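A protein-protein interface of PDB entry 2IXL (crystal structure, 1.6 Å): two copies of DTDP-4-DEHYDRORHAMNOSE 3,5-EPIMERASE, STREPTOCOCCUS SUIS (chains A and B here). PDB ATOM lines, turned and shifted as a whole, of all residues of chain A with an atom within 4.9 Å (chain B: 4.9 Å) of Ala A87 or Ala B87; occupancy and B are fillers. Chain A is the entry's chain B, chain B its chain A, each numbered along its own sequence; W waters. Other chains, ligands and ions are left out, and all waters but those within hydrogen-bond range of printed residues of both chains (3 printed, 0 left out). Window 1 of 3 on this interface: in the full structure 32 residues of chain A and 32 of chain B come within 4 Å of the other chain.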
ATOM      1  N   TRP A  35      26.461 -20.097  25.367  1.00  0.00           N
ATOM      2  CA  TRP A  35      25.112 -20.043  24.803  1.00  0.00           C
ATOM      3  C   TRP A  35      24.855 -18.809  23.926  1.00  0.00           C
ATOM      4  O   TRP A  35      25.659 -17.874  23.885  1.00  0.00           O
ATOM      5  CB  TRP A  35      24.008 -20.218  25.877  1.00  0.00           C
ATOM      6  CG  TRP A  35      24.038 -19.302  27.123  1.00  0.00           C
ATOM      7  CD1 TRP A  35      24.407 -19.667  28.391  1.00  0.00           C
ATOM      8  CD2 TRP A  35      23.644 -17.923  27.210  1.00  0.00           C
ATOM      9  NE1 TRP A  35      24.280 -18.607  29.261  1.00  0.00           N
ATOM     10  CE2 TRP A  35      23.814 -17.521  28.572  1.00  0.00           C
ATOM     11  CE3 TRP A  35      23.183 -16.982  26.281  1.00  0.00           C
ATOM     12  CZ2 TRP A  35      23.525 -16.210  29.018  1.00  0.00           C
ATOM     13  CZ3 TRP A  35      22.899 -15.675  26.723  1.00  0.00           C
ATOM     14  CH2 TRP A  35      23.073 -15.307  28.085  1.00  0.00           C
ATOM     15  N   VAL A  64      22.694  -0.670  29.639  1.00  0.00           N
ATOM     16  CA  VAL A  64      23.143  -1.858  30.399  1.00  0.00           C
ATOM     17  C   VAL A  64      23.606  -1.410  31.785  1.00  0.00           C
ATOM     18  O   VAL A  64      24.352  -0.442  31.897  1.00  0.00           O
ATOM     19  CB  VAL A  64      24.320  -2.608  29.703  1.00  0.00           C
ATOM     20  CG1 VAL A  64      24.754  -3.838  30.531  1.00  0.00           C
ATOM     21  CG2 VAL A  64      23.976  -3.013  28.246  1.00  0.00           C
ATOM     22  N   PHE A  66      25.448  -3.120  35.378  1.00  0.00           N
ATOM     23  CA  PHE A  66      26.130  -4.292  35.943  1.00  0.00           C
ATOM     24  C   PHE A  66      26.109  -4.117  37.463  1.00  0.00           C
ATOM     25  O   PHE A  66      26.508  -3.068  37.970  1.00  0.00           O
ATOM     26  CB  PHE A  66      27.553  -4.383  35.384  1.00  0.00           C
ATOM     27  CG  PHE A  66      28.256  -5.686  35.681  1.00  0.00           C
ATOM     28  CD1 PHE A  66      27.773  -6.885  35.173  1.00  0.00           C
ATOM     29  CD2 PHE A  66      29.395  -5.712  36.476  1.00  0.00           C
ATOM     30  CE1 PHE A  66      28.419  -8.087  35.439  1.00  0.00           C
ATOM     31  CE2 PHE A  66      30.048  -6.916  36.748  1.00  0.00           C
ATOM     32  CZ  PHE A  66      29.558  -8.100  36.225  1.00  0.00           C
ATOM     33  N   SER A  85      15.656  -7.478  30.017  1.00  0.00           N
ATOM     34  CA  SER A  85      16.124  -8.878  30.218  1.00  0.00           C
ATOM     35  C   SER A  85      17.516  -8.890  30.850  1.00  0.00           C
ATOM     36  O   SER A  85      18.088  -7.823  31.170  1.00  0.00           O
ATOM     37  CB  SER A  85      16.097  -9.718  28.911  1.00  0.00           C
ATOM     38  OG  SER A  85      16.292 -11.130  29.152  1.00  0.00           O
ATOM     39  N   VAL A  86      18.021 -10.103  31.080  1.00  0.00           N
ATOM     40  CA  VAL A  86      19.358 -10.339  31.635  1.00  0.00           C
ATOM     41  C   VAL A  86      20.287 -10.785  30.496  1.00  0.00           C
ATOM     42  O   VAL A  86      19.903 -11.625  29.671  1.00  0.00           O
ATOM     43  CB  VAL A  86      19.303 -11.390  32.776  1.00  0.00           C
ATOM     44  CG1 VAL A  86      20.687 -11.897  33.143  1.00  0.00           C
ATOM     45  CG2 VAL A  86      18.586 -10.797  34.009  1.00  0.00           C
ATOM     46  N   ALA A  87      21.498 -10.221  30.452  1.00  0.00           N
ATOM     47  CA  ALA A  87      22.447 -10.484  29.339  1.00  0.00           C
ATOM     48  C   ALA A  87      23.595 -11.449  29.681  1.00  0.00           C
ATOM     49  O   ALA A  87      24.375 -11.818  28.806  1.00  0.00           O
ATOM     50  CB  ALA A  87      23.017  -9.160  28.782  1.00  0.00           C
ATOM     51  N   ASP A  88      23.715 -11.846  30.943  1.00  0.00           N
ATOM     52  CA  ASP A  88      24.755 -12.804  31.335  1.00  0.00           C
ATOM     53  C   ASP A  88      24.144 -14.014  32.064  1.00  0.00           C
ATOM     54  O   ASP A  88      22.959 -14.302  31.879  1.00  0.00           O
ATOM     55  CB  ASP A  88      25.884 -12.126  32.132  1.00  0.00           C
ATOM     56  CG  ASP A  88      25.455 -11.674  33.530  1.00  0.00           C
ATOM     57  OD1 ASP A  88      24.242 -11.713  33.850  1.00  0.00           O
ATOM     58  OD2 ASP A  88      26.356 -11.265  34.305  1.00  0.00           O
ATOM     59  N   GLY A  89      24.930 -14.721  32.878  1.00  0.00           N
ATOM     60  CA  GLY A  89      24.406 -15.880  33.607  1.00  0.00           C
ATOM     61  C   GLY A  89      23.739 -15.583  34.949  1.00  0.00           C
ATOM     62  O   GLY A  89      23.484 -16.506  35.735  1.00  0.00           O
ATOM     63  N   ALA A 137      24.226  -8.737  34.579  1.00  0.00           N
ATOM     64  CA  ALA A 137      24.161  -7.730  33.520  1.00  0.00           C
ATOM     65  C   ALA A 137      22.696  -7.593  33.095  1.00  0.00           C
ATOM     66  O   ALA A 137      22.061  -8.569  32.671  1.00  0.00           O
ATOM     67  CB  ALA A 137      25.041  -8.153  32.334  1.00  0.00           C
ATOM     68  N   TYR A 138      22.160  -6.388  33.246  1.00  0.00           N
ATOM     69  CA  TYR A 138      20.735  -6.132  33.046  1.00  0.00           C
ATOM     70  C   TYR A 138      20.616  -5.163  31.867  1.00  0.00           C
ATOM     71  O   TYR A 138      21.111  -4.033  31.920  1.00  0.00           O
ATOM     72  CB  TYR A 138      20.177  -5.547  34.350  1.00  0.00           C
ATOM     73  CG  TYR A 138      18.697  -5.234  34.439  1.00  0.00           C
ATOM     74  CD1 TYR A 138      17.807  -6.133  35.031  1.00  0.00           C
ATOM     75  CD2 TYR A 138      18.204  -3.992  34.033  1.00  0.00           C
ATOM     76  CE1 TYR A 138      16.417  -5.825  35.158  1.00  0.00           C
ATOM     77  CE2 TYR A 138      16.834  -3.669  34.160  1.00  0.00           C
ATOM     78  CZ  TYR A 138      15.959  -4.582  34.740  1.00  0.00           C
ATOM     79  OH  TYR A 138      14.617  -4.262  34.870  1.00  0.00           O
ATOM     80  N   SER A 139      19.977  -5.616  30.792  1.00  0.00           N
ATOM     81  CA  SER A 139      20.019  -4.882  29.518  1.00  0.00           C
ATOM     82  C   SER A 139      18.610  -4.529  29.079  1.00  0.00           C
ATOM     83  O   SER A 139      17.729  -5.381  29.081  1.00  0.00           O
ATOM     84  CB  SER A 139      20.721  -5.738  28.443  1.00  0.00           C
ATOM     85  OG  SER A 139      20.798  -5.080  27.172  1.00  0.00           O
ATOM     86  N   TRP B  35      28.076  -0.541  37.792  1.00  0.00           N
ATOM     87  CA  TRP B  35      28.098   0.530  36.786  1.00  0.00           C
ATOM     88  C   TRP B  35      26.852   0.594  35.880  1.00  0.00           C
ATOM     89  O   TRP B  35      26.006  -0.304  35.897  1.00  0.00           O
ATOM     90  CB  TRP B  35      29.399   0.511  35.952  1.00  0.00           C
ATOM     91  CG  TRP B  35      29.833  -0.800  35.323  1.00  0.00           C
ATOM     92  CD1 TRP B  35      30.869  -1.601  35.744  1.00  0.00           C
ATOM     93  CD2 TRP B  35      29.302  -1.429  34.135  1.00  0.00           C
ATOM     94  NE1 TRP B  35      30.999  -2.693  34.905  1.00  0.00           N
ATOM     95  CE2 TRP B  35      30.054  -2.608  33.914  1.00  0.00           C
ATOM     96  CE3 TRP B  35      28.250  -1.123  33.250  1.00  0.00           C
ATOM     97  CZ2 TRP B  35      29.793  -3.478  32.845  1.00  0.00           C
ATOM     98  CZ3 TRP B  35      27.985  -1.998  32.184  1.00  0.00           C
ATOM     99  CH2 TRP B  35      28.766  -3.159  31.996  1.00  0.00           C
ATOM    100  N   VAL B  64      22.480 -11.868  21.992  1.00  0.00           N
ATOM    101  CA  VAL B  64      23.462 -11.951  23.087  1.00  0.00           C
ATOM    102  C   VAL B  64      24.071 -13.343  23.086  1.00  0.00           C
ATOM    103  O   VAL B  64      23.348 -14.329  22.979  1.00  0.00           O
ATOM    104  CB  VAL B  64      22.818 -11.673  24.481  1.00  0.00           C
ATOM    105  CG1 VAL B  64      23.848 -11.848  25.606  1.00  0.00           C
ATOM    106  CG2 VAL B  64      22.190 -10.272  24.528  1.00  0.00           C
ATOM    107  N   PHE B  66      27.014 -15.752  25.334  1.00  0.00           N
ATOM    108  CA  PHE B  66      27.813 -15.865  26.541  1.00  0.00           C
ATOM    109  C   PHE B  66      28.876 -16.925  26.257  1.00  0.00           C
ATOM    110  O   PHE B  66      28.551 -18.006  25.767  1.00  0.00           O
ATOM    111  CB  PHE B  66      26.917 -16.281  27.716  1.00  0.00           C
ATOM    112  CG  PHE B  66      27.576 -16.149  29.077  1.00  0.00           C
ATOM    113  CD1 PHE B  66      27.881 -14.895  29.607  1.00  0.00           C
ATOM    114  CD2 PHE B  66      27.879 -17.287  29.823  1.00  0.00           C
ATOM    115  CE1 PHE B  66      28.500 -14.771  30.873  1.00  0.00           C
ATOM    116  CE2 PHE B  66      28.497 -17.176  31.078  1.00  0.00           C
ATOM    117  CZ  PHE B  66      28.798 -15.908  31.601  1.00  0.00           C
ATOM    118  N   SER B  85      29.120  -4.734  21.214  1.00  0.00           N
ATOM    119  CA  SER B  85      29.858  -4.361  22.452  1.00  0.00           C
ATOM    120  C   SER B  85      29.777  -5.498  23.463  1.00  0.00           C
ATOM    121  O   SER B  85      29.238  -6.574  23.157  1.00  0.00           O
ATOM    122  CB  SER B  85      29.358  -3.031  23.072  1.00  0.00           C
ATOM    123  OG  SER B  85      30.152  -2.612  24.209  1.00  0.00           O
ATOM    124  N   VAL B  86      30.328  -5.248  24.650  1.00  0.00           N
ATOM    125  CA  VAL B  86      30.355  -6.203  25.759  1.00  0.00           C
ATOM    126  C   VAL B  86      29.384  -5.694  26.842  1.00  0.00           C
ATOM    127  O   VAL B  86      29.365  -4.487  27.141  1.00  0.00           O
ATOM    128  CB  VAL B  86      31.809  -6.360  26.319  1.00  0.00           C
ATOM    129  CG1 VAL B  86      31.825  -7.058  27.680  1.00  0.00           C
ATOM    130  CG2 VAL B  86      32.712  -7.114  25.317  1.00  0.00           C
ATOM    131  N   ALA B  87      28.586  -6.603  27.410  1.00  0.00           N
ATOM    132  CA  ALA B  87      27.522  -6.264  28.374  1.00  0.00           C
ATOM    133  C   ALA B  87      27.844  -6.546  29.855  1.00  0.00           C
ATOM    134  O   ALA B  87      27.089  -6.113  30.748  1.00  0.00           O
ATOM    135  CB  ALA B  87      26.201  -6.955  27.979  1.00  0.00           C
ATOM    136  N   ASP B  88      28.936  -7.264  30.122  1.00  0.00           N
ATOM    137  CA  ASP B  88      29.367  -7.552  31.498  1.00  0.00           C
ATOM    138  C   ASP B  88      30.800  -7.035  31.758  1.00  0.00           C
ATOM    139  O   ASP B  88      31.250  -6.118  31.065  1.00  0.00           O
ATOM    140  CB  ASP B  88      29.187  -9.046  31.837  1.00  0.00           C
ATOM    141  CG  ASP B  88      30.159  -9.975  31.089  1.00  0.00           C
ATOM    142  OD1 ASP B  88      30.902  -9.533  30.173  1.00  0.00           O
ATOM    143  OD2 ASP B  88      30.168 -11.189  31.437  1.00  0.00           O
ATOM    144  N   GLY B  89      31.506  -7.613  32.738  1.00  0.00           N
ATOM    145  CA  GLY B  89      32.876  -7.177  33.041  1.00  0.00           C
ATOM    146  C   GLY B  89      33.990  -7.844  32.233  1.00  0.00           C
ATOM    147  O   GLY B  89      35.172  -7.712  32.576  1.00  0.00           O
ATOM    148  N   ALA B 137      29.916 -11.615  28.161  1.00  0.00           N
ATOM    149  CA  ALA B 137      28.604 -11.438  27.518  1.00  0.00           C
ATOM    150  C   ALA B 137      28.766 -10.440  26.380  1.00  0.00           C
ATOM    151  O   ALA B 137      29.212  -9.323  26.592  1.00  0.00           O
ATOM    152  CB  ALA B 137      27.562 -10.928  28.520  1.00  0.00           C
ATOM    153  N   TYR B 138      28.409 -10.864  25.170  1.00  0.00           N
ATOM    154  CA  TYR B 138      28.654 -10.101  23.949  1.00  0.00           C
ATOM    155  C   TYR B 138      27.289  -9.781  23.330  1.00  0.00           C
ATOM    156  O   TYR B 138      26.512 -10.683  23.011  1.00  0.00           O
ATOM    157  CB  TYR B 138      29.515 -10.990  23.055  1.00  0.00           C
ATOM    158  CG  TYR B 138      30.013 -10.465  21.730  1.00  0.00           C
ATOM    159  CD1 TYR B 138      31.285  -9.896  21.619  1.00  0.00           C
ATOM    160  CD2 TYR B 138      29.256 -10.623  20.571  1.00  0.00           C
ATOM    161  CE1 TYR B 138      31.787  -9.461  20.374  1.00  0.00           C
ATOM    162  CE2 TYR B 138      29.733 -10.197  19.330  1.00  0.00           C
ATOM    163  CZ  TYR B 138      30.999  -9.622  19.238  1.00  0.00           C
ATOM    164  OH  TYR B 138      31.442  -9.210  17.998  1.00  0.00           O
ATOM    165  N   SER B 139      26.972  -8.494  23.207  1.00  0.00           N
ATOM    166  CA  SER B 139      25.614  -8.102  22.848  1.00  0.00           C
ATOM    167  C   SER B 139      25.665  -7.249  21.605  1.00  0.00           C
ATOM    168  O   SER B 139      26.501  -6.341  21.506  1.00  0.00           O
ATOM    169  CB  SER B 139      24.959  -7.335  24.009  1.00  0.00           C
ATOM    170  OG  SER B 139      23.663  -6.859  23.656  1.00  0.00           O
HETATM  171  O   HOH W   1      28.918 -11.870  33.950  1.00  0.00           O
HETATM  172  O   HOH W   2      23.294  -4.572  25.354  1.00  0.00           O
HETATM  173  O   HOH W   3      20.938  -7.301  25.437  1.00  0.00           O
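The backbone carbonyl oxygen (O) of Trp B35 sits at hydrogen-bond distance from the backbone NH (N) of Phe A66 (2.9 Å).
The backbone NH (N) of Phe B66 is in hydrogen-bond range of the backbone carbonyl oxygen (O) of Trp A35.
The backbone NH (N) of Ala B87 is in hydrogen-bond range of the backbone carbonyl oxygen (O) of Ala B137 (2.9 Å).
OD1 of Asp B88 sits at hydrogen-bond distance from N of Ala B137.
N of Ala A87 sits at hydrogen-bond distance from O of Ala A137, at 2.8 Å.
N of Ala A137 sits at hydrogen-bond distance from OD1 of Asp A88 (3.1 Å).
Val A64 touches Trp B35.
Val A64 touches Ala B87.
CE1 of Phe A66 touches CB of Asp B88 (3.8 Å).
CG1 of Val B64 touches O of Ala A87, at 3.2 Å.
CB of Ala A87 touches CB of Ala B87 (3.96 Å).
CB of Ala B137 touches O of Ala A87 (3.3 Å).
CB of Asp A88 touches CE1 of Phe B66, 3.9 Å away.
Ala A137 touches Ala B87 (CB to O, 3.3 Å).
Printed residues of chain B within 4 Å of Phe A66: Trp B35 and Asp B88.
Of the printed residues of chain A, Phe B66 touches Trp A35 (2.9 Å) and Asp A88 (3.9 Å).
The nearest residue of chain A that does not touch Ala B87 is Phe A66 (4.5 Å).
Of the 11 printed residues of chain B, 6 touch a printed residue of chain A.
Printed residues of chain A that touch a printed residue of chain B: Trp A35, Val A64, Phe A66, Ala A87, Asp A88 and Ala A137.
Among the printed residues, no Asp or Glu carboxylate lies within 4 Å of a Lys or Arg side-chain nitrogen of the other chain.
Trp A35 touches Phe B66, and with the chains exchanged Phe A66 touches Trp B35.
Val A64 touches Ala B87, and with the chains exchanged Ala A87 touches Val B64.
Phe A66 touches Asp B88, and with the chains exchanged Asp A88 touches Phe B66.
Ala A87 touches Ala B137, and with the chains exchanged Ala A137 touches Ala B87.
Positions printed for both chains: 35, 64, 66, 85, 86, 87, 88, 89, 137, 138 and 139.
Of the 10 pairs that touch across the chains among the printed residues, 9 have their exchanged pair printed and touching as well.
Water W1 lies within hydrogen-bond range of the side-chain carboxylate of Asp A88 and the side-chain carboxylate of Asp B88.
Water W3 lies within hydrogen-bond range of the side-chain hydroxyl (OG) of Ser A139 (2.8 Å) and the side-chain hydroxyl (OG) of Ser B139 (3.3 Å).
Water W2 lies within hydrogen-bond range of the side-chain hydroxyl of Ser B139 (2.9 Å) and the side-chain hydroxyl of Ser A139 (3.1 Å).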
